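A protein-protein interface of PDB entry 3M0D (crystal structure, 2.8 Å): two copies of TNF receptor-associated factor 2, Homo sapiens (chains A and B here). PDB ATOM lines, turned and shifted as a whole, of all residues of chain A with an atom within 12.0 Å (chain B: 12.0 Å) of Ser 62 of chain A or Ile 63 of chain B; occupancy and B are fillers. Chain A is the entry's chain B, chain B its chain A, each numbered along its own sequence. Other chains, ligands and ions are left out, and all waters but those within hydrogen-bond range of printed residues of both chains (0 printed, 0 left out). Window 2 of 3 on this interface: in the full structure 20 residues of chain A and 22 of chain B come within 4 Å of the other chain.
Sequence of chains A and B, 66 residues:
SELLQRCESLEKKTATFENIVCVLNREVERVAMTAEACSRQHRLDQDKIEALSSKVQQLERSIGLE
Hydrophobic or aromatic side chains of chain A within 4 Å of the printed part of chain B: Val 56 and Leu 59. Among the printed residues, 5 pairs touch across the chains.
Among the printed residues, pairs that only touch across the chains: Leu 59 of chain A with Leu 59 of chain B (3.8 Å), Lys 55 of chain A with Glu 60 of chain B (3.9 Å), Val 56 of chain A with Val 56 of chain B (3.9 Å), Lys 55 of chain A with Val 56 of chain B (3.9 Å) and Ser 62 of chain A with Ile 63 of chain B (3.9 Å).
Printed residues of chain B within 4 Å of Val 56 of chain A: Val 56. Gln 57 of chain A touches none of the printed residues of chain B. Ser 62 of chain A touches just one residue of chain B: Ile 63. Lys 55 of chain B touches none of the printed residues of chain A. Leu 59 of chain B touches just one residue of chain A: Leu 59 (3.8 Å). Of the printed residues of chain A, Glu 60 of chain B touches Lys 55. No residue of chain A comes within 4 Å of Ser 62 of chain B. Of chain A, only Ser 62 (3.9 Å) comes within 4 Å of Ile 63 of chain B. Gly 64 of chain B touches none of the printed residues of chain A. The nearest residue of chain B that does not touch Ser 62 of chain A is Gly 64 of chain B (7.2 Å). The nearest residue of chain A that does not touch Ile 63 of chain B is Leu 59 of chain A (4.04 Å).
Lys 55 of chain A touches Val 56 of chain B, but with the chains exchanged Val 56 of chain A does not touch Lys 55 of chain B (7.6 Å). Lys 55 of chain A touches Glu 60 of chain B, but with the chains exchanged Glu 60 of chain A does not touch Lys 55 of chain B (11.0 Å). Val 56 of chain B touches its own counterpart, Val 56 of chain A. Leu 59 of chain B touches its own counterpart, Leu 59 of chain A. Of the 5 pairs that touch across the chains among the printed residues, 2 have their exchanged pair printed and touching as well.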
ATOM      1  N   SER A  53     -27.836  -9.680  19.106  1.00  0.00           N
ATOM      2  CA  SER A  53     -28.487  -8.678  19.924  1.00  0.00           C
ATOM      3  C   SER A  53     -27.714  -7.372  19.789  1.00  0.00           C
ATOM      4  O   SER A  53     -28.293  -6.294  19.645  1.00  0.00           O
ATOM      5  CB  SER A  53     -28.506  -9.141  21.376  1.00  0.00           C
ATOM      6  OG  SER A  53     -29.445  -8.397  22.110  1.00  0.00           O
ATOM      7  N   SER A  54     -26.389  -7.493  19.826  1.00  0.00           N
ATOM      8  CA  SER A  54     -25.479  -6.365  19.631  1.00  0.00           C
ATOM      9  C   SER A  54     -25.734  -5.658  18.304  1.00  0.00           C
ATOM     10  O   SER A  54     -25.835  -4.435  18.235  1.00  0.00           O
ATOM     11  CB  SER A  54     -24.032  -6.862  19.657  1.00  0.00           C
ATOM     12  OG  SER A  54     -23.150  -5.859  20.116  1.00  0.00           O
ATOM     13  N   LYS A  55     -25.824  -6.458  17.251  1.00  0.00           N
ATOM     14  CA  LYS A  55     -26.004  -5.957  15.910  1.00  0.00           C
ATOM     15  C   LYS A  55     -27.328  -5.225  15.721  1.00  0.00           C
ATOM     16  O   LYS A  55     -27.364  -4.187  15.046  1.00  0.00           O
ATOM     17  CB  LYS A  55     -25.844  -7.099  14.906  1.00  0.00           C
ATOM     18  CG  LYS A  55     -24.415  -7.648  14.827  1.00  0.00           C
ATOM     19  CD  LYS A  55     -24.319  -8.855  13.897  1.00  0.00           C
ATOM     20  CE  LYS A  55     -22.916  -9.471  13.883  1.00  0.00           C
ATOM     21  NZ  LYS A  55     -21.900  -8.620  13.186  1.00  0.00           N
ATOM     22  N   VAL A  56     -28.412  -5.740  16.305  1.00  0.00           N
ATOM     23  CA  VAL A  56     -29.697  -5.028  16.222  1.00  0.00           C
ATOM     24  C   VAL A  56     -29.759  -3.748  17.058  1.00  0.00           C
ATOM     25  O   VAL A  56     -30.594  -2.897  16.800  1.00  0.00           O
ATOM     26  CB  VAL A  56     -30.927  -5.884  16.597  1.00  0.00           C
ATOM     27  CG1 VAL A  56     -31.154  -7.004  15.592  1.00  0.00           C
ATOM     28  CG2 VAL A  56     -30.764  -6.421  17.987  1.00  0.00           C
ATOM     29  N   GLN A  57     -28.917  -3.607  18.073  1.00  0.00           N
ATOM     30  CA  GLN A  57     -28.910  -2.353  18.800  1.00  0.00           C
ATOM     31  C   GLN A  57     -28.234  -1.324  17.902  1.00  0.00           C
ATOM     32  O   GLN A  57     -28.620  -0.162  17.864  1.00  0.00           O
ATOM     33  CB  GLN A  57     -28.184  -2.483  20.137  1.00  0.00           C
ATOM     34  CG  GLN A  57     -28.595  -1.431  21.161  1.00  0.00           C
ATOM     35  CD  GLN A  57     -27.750  -1.475  22.430  1.00  0.00           C
ATOM     36  OE1 GLN A  57     -26.535  -1.255  22.398  1.00  0.00           O
ATOM     37  NE2 GLN A  57     -28.394  -1.759  23.556  1.00  0.00           N
ATOM     38  N   GLN A  58     -27.230  -1.780  17.162  1.00  0.00           N
ATOM     39  CA  GLN A  58     -26.468  -0.915  16.279  1.00  0.00           C
ATOM     40  C   GLN A  58     -27.323  -0.407  15.121  1.00  0.00           C
ATOM     41  O   GLN A  58     -27.282   0.778  14.781  1.00  0.00           O
ATOM     42  CB  GLN A  58     -25.211  -1.634  15.760  1.00  0.00           C
ATOM     43  CG  GLN A  58     -24.175  -0.681  15.182  1.00  0.00           C
ATOM     44  CD  GLN A  58     -24.106   0.641  15.954  1.00  0.00           C
ATOM     45  OE1 GLN A  58     -23.725   0.667  17.129  1.00  0.00           O
ATOM     46  NE2 GLN A  58     -24.490   1.740  15.298  1.00  0.00           N
ATOM     47  N   LEU A  59     -28.085  -1.308  14.512  1.00  0.00           N
ATOM     48  CA  LEU A  59     -29.022  -0.926  13.459  1.00  0.00           C
ATOM     49  C   LEU A  59     -30.066   0.063  13.960  1.00  0.00           C
ATOM     50  O   LEU A  59     -30.341   1.066  13.303  1.00  0.00           O
ATOM     51  CB  LEU A  59     -29.711  -2.156  12.876  1.00  0.00           C
ATOM     52  CG  LEU A  59     -28.857  -3.011  11.944  1.00  0.00           C
ATOM     53  CD1 LEU A  59     -29.552  -4.282  11.490  1.00  0.00           C
ATOM     54  CD2 LEU A  59     -28.476  -2.182  10.737  1.00  0.00           C
ATOM     55  N   GLU A  60     -30.646  -0.222  15.123  1.00  0.00           N
ATOM     56  CA  GLU A  60     -31.609   0.683  15.742  1.00  0.00           C
ATOM     57  C   GLU A  60     -31.044   2.083  15.988  1.00  0.00           C
ATOM     58  O   GLU A  60     -31.750   3.078  15.825  1.00  0.00           O
ATOM     59  CB  GLU A  60     -32.137   0.094  17.047  1.00  0.00           C
ATOM     60  CG  GLU A  60     -33.168  -0.996  16.830  1.00  0.00           C
ATOM     61  CD  GLU A  60     -33.729  -1.532  18.126  1.00  0.00           C
ATOM     62  OE1 GLU A  60     -33.116  -1.266  19.185  1.00  0.00           O
ATOM     63  OE2 GLU A  60     -34.781  -2.213  18.067  1.00  0.00           O
ATOM     64  N   ARG A  61     -29.777   2.155  16.387  1.00  0.00           N
ATOM     65  CA  ARG A  61     -29.092   3.433  16.540  1.00  0.00           C
ATOM     66  C   ARG A  61     -28.734   4.052  15.182  1.00  0.00           C
ATOM     67  O   ARG A  61     -28.660   5.278  15.051  1.00  0.00           O
ATOM     68  CB  ARG A  61     -27.847   3.293  17.434  1.00  0.00           C
ATOM     69  CG  ARG A  61     -28.179   3.289  18.917  1.00  0.00           C
ATOM     70  CD  ARG A  61     -27.125   2.581  19.758  1.00  0.00           C
ATOM     71  NE  ARG A  61     -27.633   2.309  21.102  1.00  0.00           N
ATOM     72  CZ  ARG A  61     -26.873   2.066  22.164  1.00  0.00           C
ATOM     73  NH1 ARG A  61     -25.548   2.062  22.049  1.00  0.00           N
ATOM     74  NH2 ARG A  61     -27.443   1.837  23.345  1.00  0.00           N
ATOM     75  N   SER A  62     -28.519   3.217  14.173  1.00  0.00           N
ATOM     76  CA  SER A  62     -28.228   3.751  12.846  1.00  0.00           C
ATOM     77  C   SER A  62     -29.486   4.216  12.110  1.00  0.00           C
ATOM     78  O   SER A  62     -29.408   5.028  11.194  1.00  0.00           O
ATOM     79  CB  SER A  62     -27.401   2.776  12.004  1.00  0.00           C
ATOM     80  OG  SER A  62     -26.017   2.967  12.223  1.00  0.00           O
ATOM     81  N   ILE A  63     -30.638   3.749  12.594  1.00  0.00           N
ATOM     82  CA  ILE A  63     -31.943   4.108  12.037  1.00  0.00           C
ATOM     83  C   ILE A  63     -32.873   4.860  13.008  1.00  0.00           C
ATOM     84  O   ILE A  63     -32.873   6.091  13.039  1.00  0.00           O
ATOM     85  CB  ILE A  63     -32.685   2.865  11.504  1.00  0.00           C
ATOM     86  CG1 ILE A  63     -31.810   2.113  10.498  1.00  0.00           C
ATOM     87  CG2 ILE A  63     -34.010   3.265  10.872  1.00  0.00           C
ATOM     88  CD1 ILE A  63     -32.571   1.111   9.656  1.00  0.00           C
ATOM     89  N   GLY A  64     -33.649   4.113  13.784  1.00  0.00           N
ATOM     90  CA  GLY A  64     -34.568   4.703  14.740  1.00  0.00           C
ATOM     91  C   GLY A  64     -35.882   3.951  14.822  1.00  0.00           C
ATOM     92  O   GLY A  64     -36.630   4.094  15.788  1.00  0.00           O
ATOM     93  N   SER B  54     -29.380 -13.991   9.064  1.00  0.00           N
ATOM     94  CA  SER B  54     -29.541 -13.815   7.637  1.00  0.00           C
ATOM     95  C   SER B  54     -30.270 -12.483   7.362  1.00  0.00           C
ATOM     96  O   SER B  54     -29.903 -11.731   6.446  1.00  0.00           O
ATOM     97  CB  SER B  54     -30.310 -15.006   7.057  1.00  0.00           C
ATOM     98  OG  SER B  54     -30.070 -15.169   5.674  1.00  0.00           O
ATOM     99  N   LYS B  55     -31.289 -12.183   8.166  1.00  0.00           N
ATOM    100  CA  LYS B  55     -32.047 -10.943   7.991  1.00  0.00           C
ATOM    101  C   LYS B  55     -31.271  -9.722   8.472  1.00  0.00           C
ATOM    102  O   LYS B  55     -31.502  -8.604   8.001  1.00  0.00           O
ATOM    103  CB  LYS B  55     -33.394 -11.005   8.716  1.00  0.00           C
ATOM    104  CG  LYS B  55     -34.373 -12.031   8.171  1.00  0.00           C
ATOM    105  CD  LYS B  55     -35.645 -12.068   9.019  1.00  0.00           C
ATOM    106  CE  LYS B  55     -36.593 -13.181   8.587  1.00  0.00           C
ATOM    107  NZ  LYS B  55     -37.295 -12.862   7.309  1.00  0.00           N
ATOM    108  N   VAL B  56     -30.362  -9.928   9.422  1.00  0.00           N
ATOM    109  CA  VAL B  56     -29.557  -8.826   9.939  1.00  0.00           C
ATOM    110  C   VAL B  56     -28.447  -8.446   8.957  1.00  0.00           C
ATOM    111  O   VAL B  56     -28.176  -7.261   8.762  1.00  0.00           O
ATOM    112  CB  VAL B  56     -29.033  -9.105  11.374  1.00  0.00           C
ATOM    113  CG1 VAL B  56     -27.942  -8.135  11.765  1.00  0.00           C
ATOM    114  CG2 VAL B  56     -30.164  -8.993  12.367  1.00  0.00           C
ATOM    115  N   GLN B  57     -27.845  -9.440   8.302  1.00  0.00           N
ATOM    116  CA  GLN B  57     -26.873  -9.165   7.252  1.00  0.00           C
ATOM    117  C   GLN B  57     -27.493  -8.381   6.085  1.00  0.00           C
ATOM    118  O   GLN B  57     -26.946  -7.369   5.663  1.00  0.00           O
ATOM    119  CB  GLN B  57     -26.227 -10.454   6.746  1.00  0.00           C
ATOM    120  CG  GLN B  57     -25.012 -10.204   5.847  1.00  0.00           C
ATOM    121  CD  GLN B  57     -24.294 -11.476   5.405  1.00  0.00           C
ATOM    122  OE1 GLN B  57     -24.918 -12.427   4.931  1.00  0.00           O
ATOM    123  NE2 GLN B  57     -22.972 -11.486   5.549  1.00  0.00           N
ATOM    124  N   GLN B  58     -28.636  -8.844   5.578  1.00  0.00           N
ATOM    125  CA  GLN B  58     -29.348  -8.161   4.492  1.00  0.00           C
ATOM    126  C   GLN B  58     -29.561  -6.672   4.795  1.00  0.00           C
ATOM    127  O   GLN B  58     -29.357  -5.813   3.923  1.00  0.00           O
ATOM    128  CB  GLN B  58     -30.689  -8.862   4.198  1.00  0.00           C
ATOM    129  CG  GLN B  58     -31.748  -7.986   3.506  1.00  0.00           C
ATOM    130  CD  GLN B  58     -31.478  -7.746   2.022  1.00  0.00           C
ATOM    131  OE1 GLN B  58     -31.017  -8.638   1.310  1.00  0.00           O
ATOM    132  NE2 GLN B  58     -31.767  -6.533   1.552  1.00  0.00           N
ATOM    133  N   LEU B  59     -29.964  -6.379   6.034  1.00  0.00           N
ATOM    134  CA  LEU B  59     -30.163  -5.005   6.502  1.00  0.00           C
ATOM    135  C   LEU B  59     -28.873  -4.178   6.536  1.00  0.00           C
ATOM    136  O   LEU B  59     -28.800  -3.086   5.968  1.00  0.00           O
ATOM    137  CB  LEU B  59     -30.774  -4.998   7.904  1.00  0.00           C
ATOM    138  CG  LEU B  59     -32.204  -5.485   8.094  1.00  0.00           C
ATOM    139  CD1 LEU B  59     -32.589  -5.452   9.567  1.00  0.00           C
ATOM    140  CD2 LEU B  59     -33.172  -4.656   7.266  1.00  0.00           C
ATOM    141  N   GLU B  60     -27.866  -4.690   7.228  1.00  0.00           N
ATOM    142  CA  GLU B  60     -26.574  -4.027   7.288  1.00  0.00           C
ATOM    143  C   GLU B  60     -26.041  -3.621   5.902  1.00  0.00           C
ATOM    144  O   GLU B  60     -25.546  -2.504   5.733  1.00  0.00           O
ATOM    145  CB  GLU B  60     -25.578  -4.932   8.008  1.00  0.00           C
ATOM    146  CG  GLU B  60     -26.061  -5.311   9.399  1.00  0.00           C
ATOM    147  CD  GLU B  60     -25.018  -6.026  10.253  1.00  0.00           C
ATOM    148  OE1 GLU B  60     -24.366  -6.974   9.750  1.00  0.00           O
ATOM    149  OE2 GLU B  60     -24.868  -5.629  11.436  1.00  0.00           O
ATOM    150  N   ARG B  61     -26.145  -4.533   4.930  1.00  0.00           N
ATOM    151  CA  ARG B  61     -25.738  -4.282   3.558  1.00  0.00           C
ATOM    152  C   ARG B  61     -26.553  -3.142   2.973  1.00  0.00           C
ATOM    153  O   ARG B  61     -26.037  -2.325   2.204  1.00  0.00           O
ATOM    154  CB  ARG B  61     -25.954  -5.529   2.714  1.00  0.00           C
ATOM    155  CG  ARG B  61     -24.782  -6.495   2.711  1.00  0.00           C
ATOM    156  CD  ARG B  61     -25.271  -7.918   2.497  1.00  0.00           C
ATOM    157  NE  ARG B  61     -24.196  -8.881   2.257  1.00  0.00           N
ATOM    158  CZ  ARG B  61     -23.210  -9.158   3.109  1.00  0.00           C
ATOM    159  NH1 ARG B  61     -23.124  -8.522   4.273  1.00  0.00           N
ATOM    160  NH2 ARG B  61     -22.293 -10.066   2.783  1.00  0.00           N
ATOM    161  N   SER B  62     -27.827  -3.099   3.351  1.00  0.00           N
ATOM    162  CA  SER B  62     -28.759  -2.102   2.845  1.00  0.00           C
ATOM    163  C   SER B  62     -28.342  -0.657   3.138  1.00  0.00           C
ATOM    164  O   SER B  62     -28.747   0.275   2.428  1.00  0.00           O
ATOM    165  CB  SER B  62     -30.169  -2.372   3.384  1.00  0.00           C
ATOM    166  OG  SER B  62     -30.853  -3.308   2.568  1.00  0.00           O
ATOM    167  N   ILE B  63     -27.529  -0.465   4.172  1.00  0.00           N
ATOM    168  CA  ILE B  63     -27.213   0.882   4.619  1.00  0.00           C
ATOM    169  C   ILE B  63     -25.712   1.147   4.801  1.00  0.00           C
ATOM    170  O   ILE B  63     -25.317   2.243   5.204  1.00  0.00           O
ATOM    171  CB  ILE B  63     -27.966   1.224   5.940  1.00  0.00           C
ATOM    172  CG1 ILE B  63     -27.279   0.599   7.152  1.00  0.00           C
ATOM    173  CG2 ILE B  63     -29.422   0.773   5.886  1.00  0.00           C
ATOM    174  CD1 ILE B  63     -27.846   1.100   8.460  1.00  0.00           C
ATOM    175  N   GLY B  64     -24.886   0.151   4.499  1.00  0.00           N
ATOM    176  CA  GLY B  64     -23.488   0.174   4.898  1.00  0.00           C
ATOM    177  C   GLY B  64     -23.337  -0.301   6.341  1.00  0.00           C
ATOM    178  O   GLY B  64     -23.137  -1.494   6.637  1.00  0.00           O
